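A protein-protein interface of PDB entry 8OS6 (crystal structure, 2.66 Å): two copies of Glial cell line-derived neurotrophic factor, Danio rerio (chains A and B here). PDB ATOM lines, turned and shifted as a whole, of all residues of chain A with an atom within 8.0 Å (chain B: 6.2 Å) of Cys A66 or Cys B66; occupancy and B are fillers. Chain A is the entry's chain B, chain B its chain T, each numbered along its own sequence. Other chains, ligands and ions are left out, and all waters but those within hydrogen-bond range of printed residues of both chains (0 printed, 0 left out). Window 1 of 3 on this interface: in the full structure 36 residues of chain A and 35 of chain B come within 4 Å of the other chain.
OG1 of Thr B65 lies within hydrogen-bond range of NH2 of Arg A68 (3.3 Å). The guanidinium group (NE) of Arg B68 lies within salt-bridge range of the chain-end carboxylate (OXT) of Val A99, 3.1 Å away. NE of Arg B68 sits at hydrogen-bond distance from O of Arg A64. NH1 of Arg A68 lies within hydrogen-bond range of O of Ser B63 (3.1 Å). The backbone carbonyl oxygen of Ser A63 sits at hydrogen-bond distance from the guanidinium group of Arg B68 (2.9 Å). The guanidinium group (NH2) of Arg A68 is in salt-bridge range of the chain-end carboxylate (O) of Val B99. The side-chain carboxylate (OD1) of Asp A45 is in salt-bridge range of the guanidinium group (NH1) of Arg B68 (3.2 Å). The backbone carbonyl oxygen (O) of Cys A67 sits at hydrogen-bond distance from the side-chain hydroxyl (OG) of Ser B63 (2.7 Å). SG of Cys A66 is disulfide-bonded to SG of Cys B66, 2.1 Å away. The side-chain hydroxyl (OG1) of Thr A65 sits at hydrogen-bond distance from the guanidinium group (NH2) of Arg B68 (3.2 Å).
Of chain B, only Cys B66 comes within 4 Å of Cys A66. Cys B66 touches just these residues of chain A: Ser A63 (3.9 Å) and Cys A66 (2.1 Å). Of the printed residues of chain A, Arg B68 touches Asp A45, Ser A63, Arg A64, Thr A65 and Val A99. Printed residues of chain B within 4 Å of Val A99: Arg B68 and Val B99. Of the printed residues of chain A, Thr B65 touches Arg A68. Of the printed residues of chain B, Asp A45 touches Arg B68. Of the printed residues of chain B, Arg A64 touches Arg B68 (3.1 Å). Pro A69 touches none of the printed residues of chain B. The nearest residue of chain A that does not touch Cys B66 is Arg A68 (4.9 Å).
Of the 11 printed residues of chain B, 6 touch a printed residue of chain A. Hydrophobic or aromatic side chains of chain B within 4 Å of the printed part of chain A: Val B99. Printed residues of chain A that touch a printed residue of chain B: Asp A45, Ser A63, Arg A64, Thr A65, Cys A66, Cys A67, Arg A68 and Val A99. Among the printed residues, 13 pairs touch across the chains. Among the printed residues, Asp or Glu carboxylates within 4 Å of a Lys or Arg side-chain nitrogen of the other chain: Asp A45 with Arg B68 (3.2 Å).
The backbone carbonyl oxygen (O) of Cys B66 sits at hydrogen-bond distance from the backbone NH (N) of Val B99 (2.8 Å). The side-chain sulfur (SG) of Cys A98 is disulfide-bonded to the side-chain sulfur (SG) of Cys A37 (2.0 Å). The side-chain hydroxyl of Ser A63 sits at hydrogen-bond distance from the side-chain sulfur of Cys A66. The side-chain sulfur of Cys A96 forms a disulfide with the side-chain sulfur of Cys A33, 2.0 Å away. The side-chain carboxylate of Glu A41 is in salt-bridge range of the guanidinium group of Arg A64, at 3.9 Å. N of Ala A97 sits at hydrogen-bond distance from O of Arg A68 (3.0 Å).
Ser A63 touches Cys B66. Arg A68 touches Arg B64 (NH1 to C, 3.2 Å). Val B99 touches Val A99 (CG2 to CG2, 3.8 Å).
Ser A63 touches Arg B68, and with the chains exchanged Arg A68 touches Ser B63. Thr A65 touches Arg B68, and with the chains exchanged Arg A68 touches Thr B65. Cys A67 touches Ser B63, but with the chains exchanged Ser A63 does not touch Cys B67 (4.3 Å). Val A99 touches its own counterpart, Val B99. 11 positions are printed for both chains. Of the 13 pairs that touch across the chains among the printed residues, 10 have their exchanged pair printed and touching as well.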
ATOM      1  N   CYS A   6     -24.894   4.626  34.722  1.00  0.00           N
ATOM      2  CA  CYS A   6     -25.776   3.913  33.807  1.00  0.00           C
ATOM      3  C   CYS A   6     -26.110   2.552  34.404  1.00  0.00           C
ATOM      4  O   CYS A   6     -25.211   1.759  34.697  1.00  0.00           O
ATOM      5  CB  CYS A   6     -25.111   3.760  32.441  1.00  0.00           C
ATOM      6  SG  CYS A   6     -26.196   3.158  31.115  1.00  0.00           S
ATOM      7  N   CYS A  33     -32.545   1.376  30.116  1.00  0.00           N
ATOM      8  CA  CYS A  33     -31.321   1.900  30.701  1.00  0.00           C
ATOM      9  C   CYS A  33     -31.542   3.335  31.160  1.00  0.00           C
ATOM     10  O   CYS A  33     -32.259   4.101  30.511  1.00  0.00           O
ATOM     11  CB  CYS A  33     -30.170   1.839  29.697  1.00  0.00           C
ATOM     12  SG  CYS A  33     -29.878   0.189  29.006  1.00  0.00           S
ATOM     13  N   GLY A  35     -29.270   6.383  33.732  1.00  0.00           N
ATOM     14  CA  GLY A  35     -28.236   6.748  34.671  1.00  0.00           C
ATOM     15  C   GLY A  35     -27.318   7.826  34.131  1.00  0.00           C
ATOM     16  O   GLY A  35     -27.257   8.073  32.922  1.00  0.00           O
ATOM     17  N   PRO A  36     -26.581   8.494  35.022  1.00  0.00           N
ATOM     18  CA  PRO A  36     -25.669   9.560  34.579  1.00  0.00           C
ATOM     19  C   PRO A  36     -24.334   8.994  34.111  1.00  0.00           C
ATOM     20  O   PRO A  36     -23.681   8.231  34.826  1.00  0.00           O
ATOM     21  CB  PRO A  36     -25.501  10.426  35.833  1.00  0.00           C
ATOM     22  CG  PRO A  36     -25.660   9.455  36.965  1.00  0.00           C
ATOM     23  CD  PRO A  36     -26.629   8.383  36.493  1.00  0.00           C
ATOM     24  N   CYS A  37     -23.930   9.380  32.899  1.00  0.00           N
ATOM     25  CA  CYS A  37     -22.664   8.956  32.315  1.00  0.00           C
ATOM     26  C   CYS A  37     -21.613  10.060  32.347  1.00  0.00           C
ATOM     27  O   CYS A  37     -20.784  10.159  31.434  1.00  0.00           O
ATOM     28  CB  CYS A  37     -22.877   8.480  30.877  1.00  0.00           C
ATOM     29  SG  CYS A  37     -23.736   6.905  30.736  1.00  0.00           S
ATOM     30  N   GLU A  41     -17.175  10.567  30.519  1.00  0.00           N
ATOM     31  CA  GLU A  41     -17.067  11.511  29.418  1.00  0.00           C
ATOM     32  C   GLU A  41     -15.606  11.800  29.096  1.00  0.00           C
ATOM     33  O   GLU A  41     -14.739  11.808  29.975  1.00  0.00           O
ATOM     34  CB  GLU A  41     -17.798  12.813  29.747  1.00  0.00           C
ATOM     35  CG  GLU A  41     -19.316  12.693  29.711  1.00  0.00           C
ATOM     36  CD  GLU A  41     -20.010  14.042  29.633  1.00  0.00           C
ATOM     37  OE1 GLU A  41     -19.308  15.075  29.609  1.00  0.00           O
ATOM     38  OE2 GLU A  41     -21.258  14.066  29.592  1.00  0.00           O
ATOM     39  N   ASP A  45     -16.389  15.071  24.612  1.00  0.00           N
ATOM     40  CA  ASP A  45     -17.609  15.581  25.229  1.00  0.00           C
ATOM     41  C   ASP A  45     -17.398  16.982  25.793  1.00  0.00           C
ATOM     42  O   ASP A  45     -18.268  17.850  25.650  1.00  0.00           O
ATOM     43  CB  ASP A  45     -18.084  14.626  26.325  1.00  0.00           C
ATOM     44  CG  ASP A  45     -18.491  13.266  25.783  1.00  0.00           C
ATOM     45  OD1 ASP A  45     -18.303  13.025  24.572  1.00  0.00           O
ATOM     46  OD2 ASP A  45     -19.002  12.439  26.568  1.00  0.00           O
ATOM     47  N   SER A  63     -24.528  15.236  20.128  1.00  0.00           N
ATOM     48  CA  SER A  63     -24.910  14.541  21.348  1.00  0.00           C
ATOM     49  C   SER A  63     -23.679  14.135  22.146  1.00  0.00           C
ATOM     50  O   SER A  63     -22.644  13.779  21.575  1.00  0.00           O
ATOM     51  CB  SER A  63     -25.744  13.299  21.020  1.00  0.00           C
ATOM     52  OG  SER A  63     -26.179  12.639  22.195  1.00  0.00           O
ATOM     53  N   ARG A  64     -23.801  14.190  23.470  1.00  0.00           N
ATOM     54  CA  ARG A  64     -22.745  13.739  24.365  1.00  0.00           C
ATOM     55  C   ARG A  64     -23.002  12.273  24.729  1.00  0.00           C
ATOM     56  O   ARG A  64     -23.783  11.588  24.064  1.00  0.00           O
ATOM     57  CB  ARG A  64     -22.669  14.658  25.588  1.00  0.00           C
ATOM     58  CG  ARG A  64     -22.043  16.013  25.293  1.00  0.00           C
ATOM     59  CD  ARG A  64     -21.552  16.695  26.561  1.00  0.00           C
ATOM     60  NE  ARG A  64     -22.640  17.000  27.482  1.00  0.00           N
ATOM     61  CZ  ARG A  64     -23.417  18.070  27.392  1.00  0.00           C
ATOM     62  NH1 ARG A  64     -23.272  18.952  26.416  1.00  0.00           N
ATOM     63  NH2 ARG A  64     -24.367  18.261  28.305  1.00  0.00           N
ATOM     64  N   THR A  65     -22.355  11.774  25.780  1.00  0.00           N
ATOM     65  CA  THR A  65     -22.490  10.368  26.142  1.00  0.00           C
ATOM     66  C   THR A  65     -23.938  10.032  26.482  1.00  0.00           C
ATOM     67  O   THR A  65     -24.644  10.821  27.118  1.00  0.00           O
ATOM     68  CB  THR A  65     -21.581  10.042  27.328  1.00  0.00           C
ATOM     69  OG1 THR A  65     -20.298  10.650  27.128  1.00  0.00           O
ATOM     70  CG2 THR A  65     -21.403   8.536  27.471  1.00  0.00           C
ATOM     71  N   CYS A  66     -24.380   8.849  26.054  1.00  0.00           N
ATOM     72  CA  CYS A  66     -25.742   8.378  26.267  1.00  0.00           C
ATOM     73  C   CYS A  66     -25.715   7.043  26.999  1.00  0.00           C
ATOM     74  O   CYS A  66     -24.955   6.144  26.627  1.00  0.00           O
ATOM     75  CB  CYS A  66     -26.491   8.224  24.935  1.00  0.00           C
ATOM     76  SG  CYS A  66     -26.694   9.758  23.997  1.00  0.00           S
ATOM     77  N   CYS A  67     -26.548   6.915  28.030  1.00  0.00           N
ATOM     78  CA  CYS A  67     -26.713   5.652  28.752  1.00  0.00           C
ATOM     79  C   CYS A  67     -27.692   4.793  27.965  1.00  0.00           C
ATOM     80  O   CYS A  67     -28.910   4.965  28.064  1.00  0.00           O
ATOM     81  CB  CYS A  67     -27.197   5.908  30.174  1.00  0.00           C
ATOM     82  SG  CYS A  67     -27.770   4.447  31.092  1.00  0.00           S
ATOM     83  N   ARG A  68     -27.162   3.865  27.180  1.00  0.00           N
ATOM     84  CA  ARG A  68     -27.927   3.088  26.220  1.00  0.00           C
ATOM     85  C   ARG A  68     -27.631   1.607  26.371  1.00  0.00           C
ATOM     86  O   ARG A  68     -26.638   1.222  26.997  1.00  0.00           O
ATOM     87  CB  ARG A  68     -27.601   3.537  24.786  1.00  0.00           C
ATOM     88  CG  ARG A  68     -28.305   4.813  24.365  1.00  0.00           C
ATOM     89  CD  ARG A  68     -29.747   4.535  23.982  1.00  0.00           C
ATOM     90  NE  ARG A  68     -29.832   3.729  22.770  1.00  0.00           N
ATOM     91  CZ  ARG A  68     -30.965   3.347  22.199  1.00  0.00           C
ATOM     92  NH1 ARG A  68     -32.141   3.686  22.702  1.00  0.00           N
ATOM     93  NH2 ARG A  68     -30.918   2.603  21.098  1.00  0.00           N
ATOM     94  N   PRO A  69     -28.482   0.747  25.813  1.00  0.00           N
ATOM     95  CA  PRO A  69     -28.236  -0.697  25.905  1.00  0.00           C
ATOM     96  C   PRO A  69     -27.233  -1.170  24.864  1.00  0.00           C
ATOM     97  O   PRO A  69     -27.210  -0.691  23.728  1.00  0.00           O
ATOM     98  CB  PRO A  69     -29.622  -1.304  25.654  1.00  0.00           C
ATOM     99  CG  PRO A  69     -30.286  -0.319  24.752  1.00  0.00           C
ATOM    100  CD  PRO A  69     -29.779   1.046  25.175  1.00  0.00           C
ATOM    101  N   ILE A  70     -26.399  -2.126  25.270  1.00  0.00           N
ATOM    102  CA  ILE A  70     -25.453  -2.768  24.362  1.00  0.00           C
ATOM    103  C   ILE A  70     -25.849  -4.194  24.018  1.00  0.00           C
ATOM    104  O   ILE A  70     -25.270  -4.771  23.082  1.00  0.00           O
ATOM    105  CB  ILE A  70     -24.019  -2.748  24.934  1.00  0.00           C
ATOM    106  CG1 ILE A  70     -23.985  -3.393  26.321  1.00  0.00           C
ATOM    107  CG2 ILE A  70     -23.501  -1.324  24.997  1.00  0.00           C
ATOM    108  CD1 ILE A  70     -22.582  -3.648  26.842  1.00  0.00           C
ATOM    109  N   CYS A  96     -26.608  -2.737  29.773  1.00  0.00           N
ATOM    110  CA  CYS A  96     -26.463  -1.314  29.495  1.00  0.00           C
ATOM    111  C   CYS A  96     -24.994  -0.906  29.556  1.00  0.00           C
ATOM    112  O   CYS A  96     -24.137  -1.643  30.052  1.00  0.00           O
ATOM    113  CB  CYS A  96     -27.282  -0.476  30.485  1.00  0.00           C
ATOM    114  SG  CYS A  96     -29.053  -0.858  30.541  1.00  0.00           S
ATOM    115  N   ALA A  97     -24.711   0.293  29.047  1.00  0.00           N
ATOM    116  CA  ALA A  97     -23.350   0.817  29.026  1.00  0.00           C
ATOM    117  C   ALA A  97     -23.377   2.282  28.612  1.00  0.00           C
ATOM    118  O   ALA A  97     -24.281   2.719  27.894  1.00  0.00           O
ATOM    119  CB  ALA A  97     -22.457   0.017  28.068  1.00  0.00           C
ATOM    120  N   CYS A  98     -22.373   3.028  29.073  1.00  0.00           N
ATOM    121  CA  CYS A  98     -22.216   4.428  28.692  1.00  0.00           C
ATOM    122  C   CYS A  98     -21.497   4.512  27.351  1.00  0.00           C
ATOM    123  O   CYS A  98     -20.342   4.088  27.233  1.00  0.00           O
ATOM    124  CB  CYS A  98     -21.434   5.195  29.757  1.00  0.00           C
ATOM    125  SG  CYS A  98     -22.342   5.530  31.280  1.00  0.00           S
ATOM    126  N   VAL A  99     -22.172   5.063  26.348  1.00  0.00           N
ATOM    127  CA  VAL A  99     -21.585   5.203  25.021  1.00  0.00           C
ATOM    128  C   VAL A  99     -21.883   6.594  24.468  1.00  0.00           C
ATOM    129  O   VAL A  99     -22.725   7.319  24.997  1.00  0.00           O
ATOM    130  CB  VAL A  99     -22.102   4.116  24.063  1.00  0.00           C
ATOM    131  CG1 VAL A  99     -21.968   2.739  24.699  1.00  0.00           C
ATOM    132  CG2 VAL A  99     -23.542   4.395  23.667  1.00  0.00           C
ATOM    133  OXT VAL A  99     -21.294   7.027  23.478  1.00  0.00           O
ATOM    134  N   CYS B   6     -26.562   9.573  10.373  1.00  0.00           N
ATOM    135  CA  CYS B   6     -25.510   9.950  11.312  1.00  0.00           C
ATOM    136  C   CYS B   6     -24.209  10.157  10.545  1.00  0.00           C
ATOM    137  O   CYS B   6     -23.576   9.189  10.109  1.00  0.00           O
ATOM    138  CB  CYS B   6     -25.366   8.870  12.380  1.00  0.00           C
ATOM    139  SG  CYS B   6     -24.163   9.205  13.689  1.00  0.00           S
ATOM    140  N   CYS B  37     -31.093   9.675  13.667  1.00  0.00           N
ATOM    141  CA  CYS B  37     -31.048   8.228  13.866  1.00  0.00           C
ATOM    142  C   CYS B  37     -32.474   7.718  14.072  1.00  0.00           C
ATOM    143  O   CYS B  37     -32.863   7.352  15.185  1.00  0.00           O
ATOM    144  CB  CYS B  37     -30.147   7.860  15.052  1.00  0.00           C
ATOM    145  SG  CYS B  37     -28.378   8.066  14.751  1.00  0.00           S
ATOM    146  N   SER B  63     -33.055   7.241  27.318  1.00  0.00           N
ATOM    147  CA  SER B  63     -32.505   7.805  26.093  1.00  0.00           C
ATOM    148  C   SER B  63     -32.769   6.899  24.900  1.00  0.00           C
ATOM    149  O   SER B  63     -32.643   5.674  24.993  1.00  0.00           O
ATOM    150  CB  SER B  63     -30.999   8.036  26.245  1.00  0.00           C
ATOM    151  OG  SER B  63     -30.409   7.019  27.040  1.00  0.00           O
ATOM    152  N   ARG B  64     -33.136   7.515  23.778  1.00  0.00           N
ATOM    153  CA  ARG B  64     -33.303   6.810  22.518  1.00  0.00           C
ATOM    154  C   ARG B  64     -31.951   6.732  21.806  1.00  0.00           C
ATOM    155  O   ARG B  64     -30.906   7.062  22.374  1.00  0.00           O
ATOM    156  CB  ARG B  64     -34.354   7.502  21.652  1.00  0.00           C
ATOM    157  CG  ARG B  64     -35.795   7.310  22.107  1.00  0.00           C
ATOM    158  CD  ARG B  64     -36.082   8.025  23.419  1.00  0.00           C
ATOM    159  NE  ARG B  64     -37.452   8.525  23.476  1.00  0.00           N
ATOM    160  CZ  ARG B  64     -38.014   9.060  24.550  1.00  0.00           C
ATOM    161  NH1 ARG B  64     -37.365   9.149  25.700  1.00  0.00           N
ATOM    162  NH2 ARG B  64     -39.261   9.518  24.469  1.00  0.00           N
ATOM    163  N   THR B  65     -31.959   6.310  20.544  1.00  0.00           N
ATOM    164  CA  THR B  65     -30.720   6.196  19.783  1.00  0.00           C
ATOM    165  C   THR B  65     -29.999   7.538  19.715  1.00  0.00           C
ATOM    166  O   THR B  65     -30.625   8.597  19.607  1.00  0.00           O
ATOM    167  CB  THR B  65     -31.018   5.687  18.370  1.00  0.00           C
ATOM    168  OG1 THR B  65     -31.676   4.416  18.444  1.00  0.00           O
ATOM    169  CG2 THR B  65     -29.737   5.538  17.568  1.00  0.00           C
ATOM    170  N   CYS B  66     -28.670   7.484  19.781  1.00  0.00           N
ATOM    171  CA  CYS B  66     -27.815   8.659  19.703  1.00  0.00           C
ATOM    172  C   CYS B  66     -26.837   8.504  18.545  1.00  0.00           C
ATOM    173  O   CYS B  66     -26.329   7.407  18.295  1.00  0.00           O
ATOM    174  CB  CYS B  66     -27.037   8.874  21.012  1.00  0.00           C
ATOM    175  SG  CYS B  66     -28.064   9.279  22.446  1.00  0.00           S
ATOM    176  N   CYS B  67     -26.585   9.603  17.837  1.00  0.00           N
ATOM    177  CA  CYS B  67     -25.576   9.644  16.778  1.00  0.00           C
ATOM    178  C   CYS B  67     -24.252  10.011  17.435  1.00  0.00           C
ATOM    179  O   CYS B  67     -23.991  11.181  17.726  1.00  0.00           O
ATOM    180  CB  CYS B  67     -25.973  10.640  15.696  1.00  0.00           C
ATOM    181  SG  CYS B  67     -24.698  11.006  14.464  1.00  0.00           S
ATOM    182  N   ARG B  68     -23.415   9.010  17.673  1.00  0.00           N
ATOM    183  CA  ARG B  68     -22.214   9.143  18.480  1.00  0.00           C
ATOM    184  C   ARG B  68     -21.023   8.512  17.783  1.00  0.00           C
ATOM    185  O   ARG B  68     -21.182   7.630  16.931  1.00  0.00           O
ATOM    186  CB  ARG B  68     -22.418   8.485  19.852  1.00  0.00           C
ATOM    187  CG  ARG B  68     -23.381   9.234  20.753  1.00  0.00           C
ATOM    188  CD  ARG B  68     -22.688  10.405  21.422  1.00  0.00           C
ATOM    189  NE  ARG B  68     -21.745   9.953  22.437  1.00  0.00           N
ATOM    190  CZ  ARG B  68     -20.838  10.728  23.017  1.00  0.00           C
ATOM    191  NH1 ARG B  68     -20.710  12.003  22.690  1.00  0.00           N
ATOM    192  NH2 ARG B  68     -20.036  10.209  23.941  1.00  0.00           N
ATOM    193  N   ALA B  97     -21.630   6.480  14.092  1.00  0.00           N
ATOM    194  CA  ALA B  97     -22.660   5.459  13.927  1.00  0.00           C
ATOM    195  C   ALA B  97     -23.802   5.684  14.912  1.00  0.00           C
ATOM    196  O   ALA B  97     -23.596   6.247  15.993  1.00  0.00           O
ATOM    197  CB  ALA B  97     -22.073   4.060  14.121  1.00  0.00           C
ATOM    198  N   CYS B  98     -25.009   5.255  14.548  1.00  0.00           N
ATOM    199  CA  CYS B  98     -26.141   5.337  15.463  1.00  0.00           C
ATOM    200  C   CYS B  98     -26.011   4.271  16.544  1.00  0.00           C
ATOM    201  O   CYS B  98     -25.878   3.080  16.244  1.00  0.00           O
ATOM    202  CB  CYS B  98     -27.456   5.160  14.707  1.00  0.00           C
ATOM    203  SG  CYS B  98     -27.861   6.499  13.560  1.00  0.00           S
ATOM    204  N   VAL B  99     -26.050   4.699  17.802  1.00  0.00           N
ATOM    205  CA  VAL B  99     -25.875   3.789  18.928  1.00  0.00           C
ATOM    206  C   VAL B  99     -27.127   3.770  19.798  1.00  0.00           C
ATOM    207  O   VAL B  99     -27.550   2.722  20.288  1.00  0.00           O
ATOM    208  CB  VAL B  99     -24.639   4.177  19.765  1.00  0.00           C
ATOM    209  CG1 VAL B  99     -23.369   4.014  18.941  1.00  0.00           C
ATOM    210  CG2 VAL B  99     -24.764   5.607  20.279  1.00  0.00           C
ATOM    211  OXT VAL B  99     -27.747   4.808  20.030  1.00  0.00           O
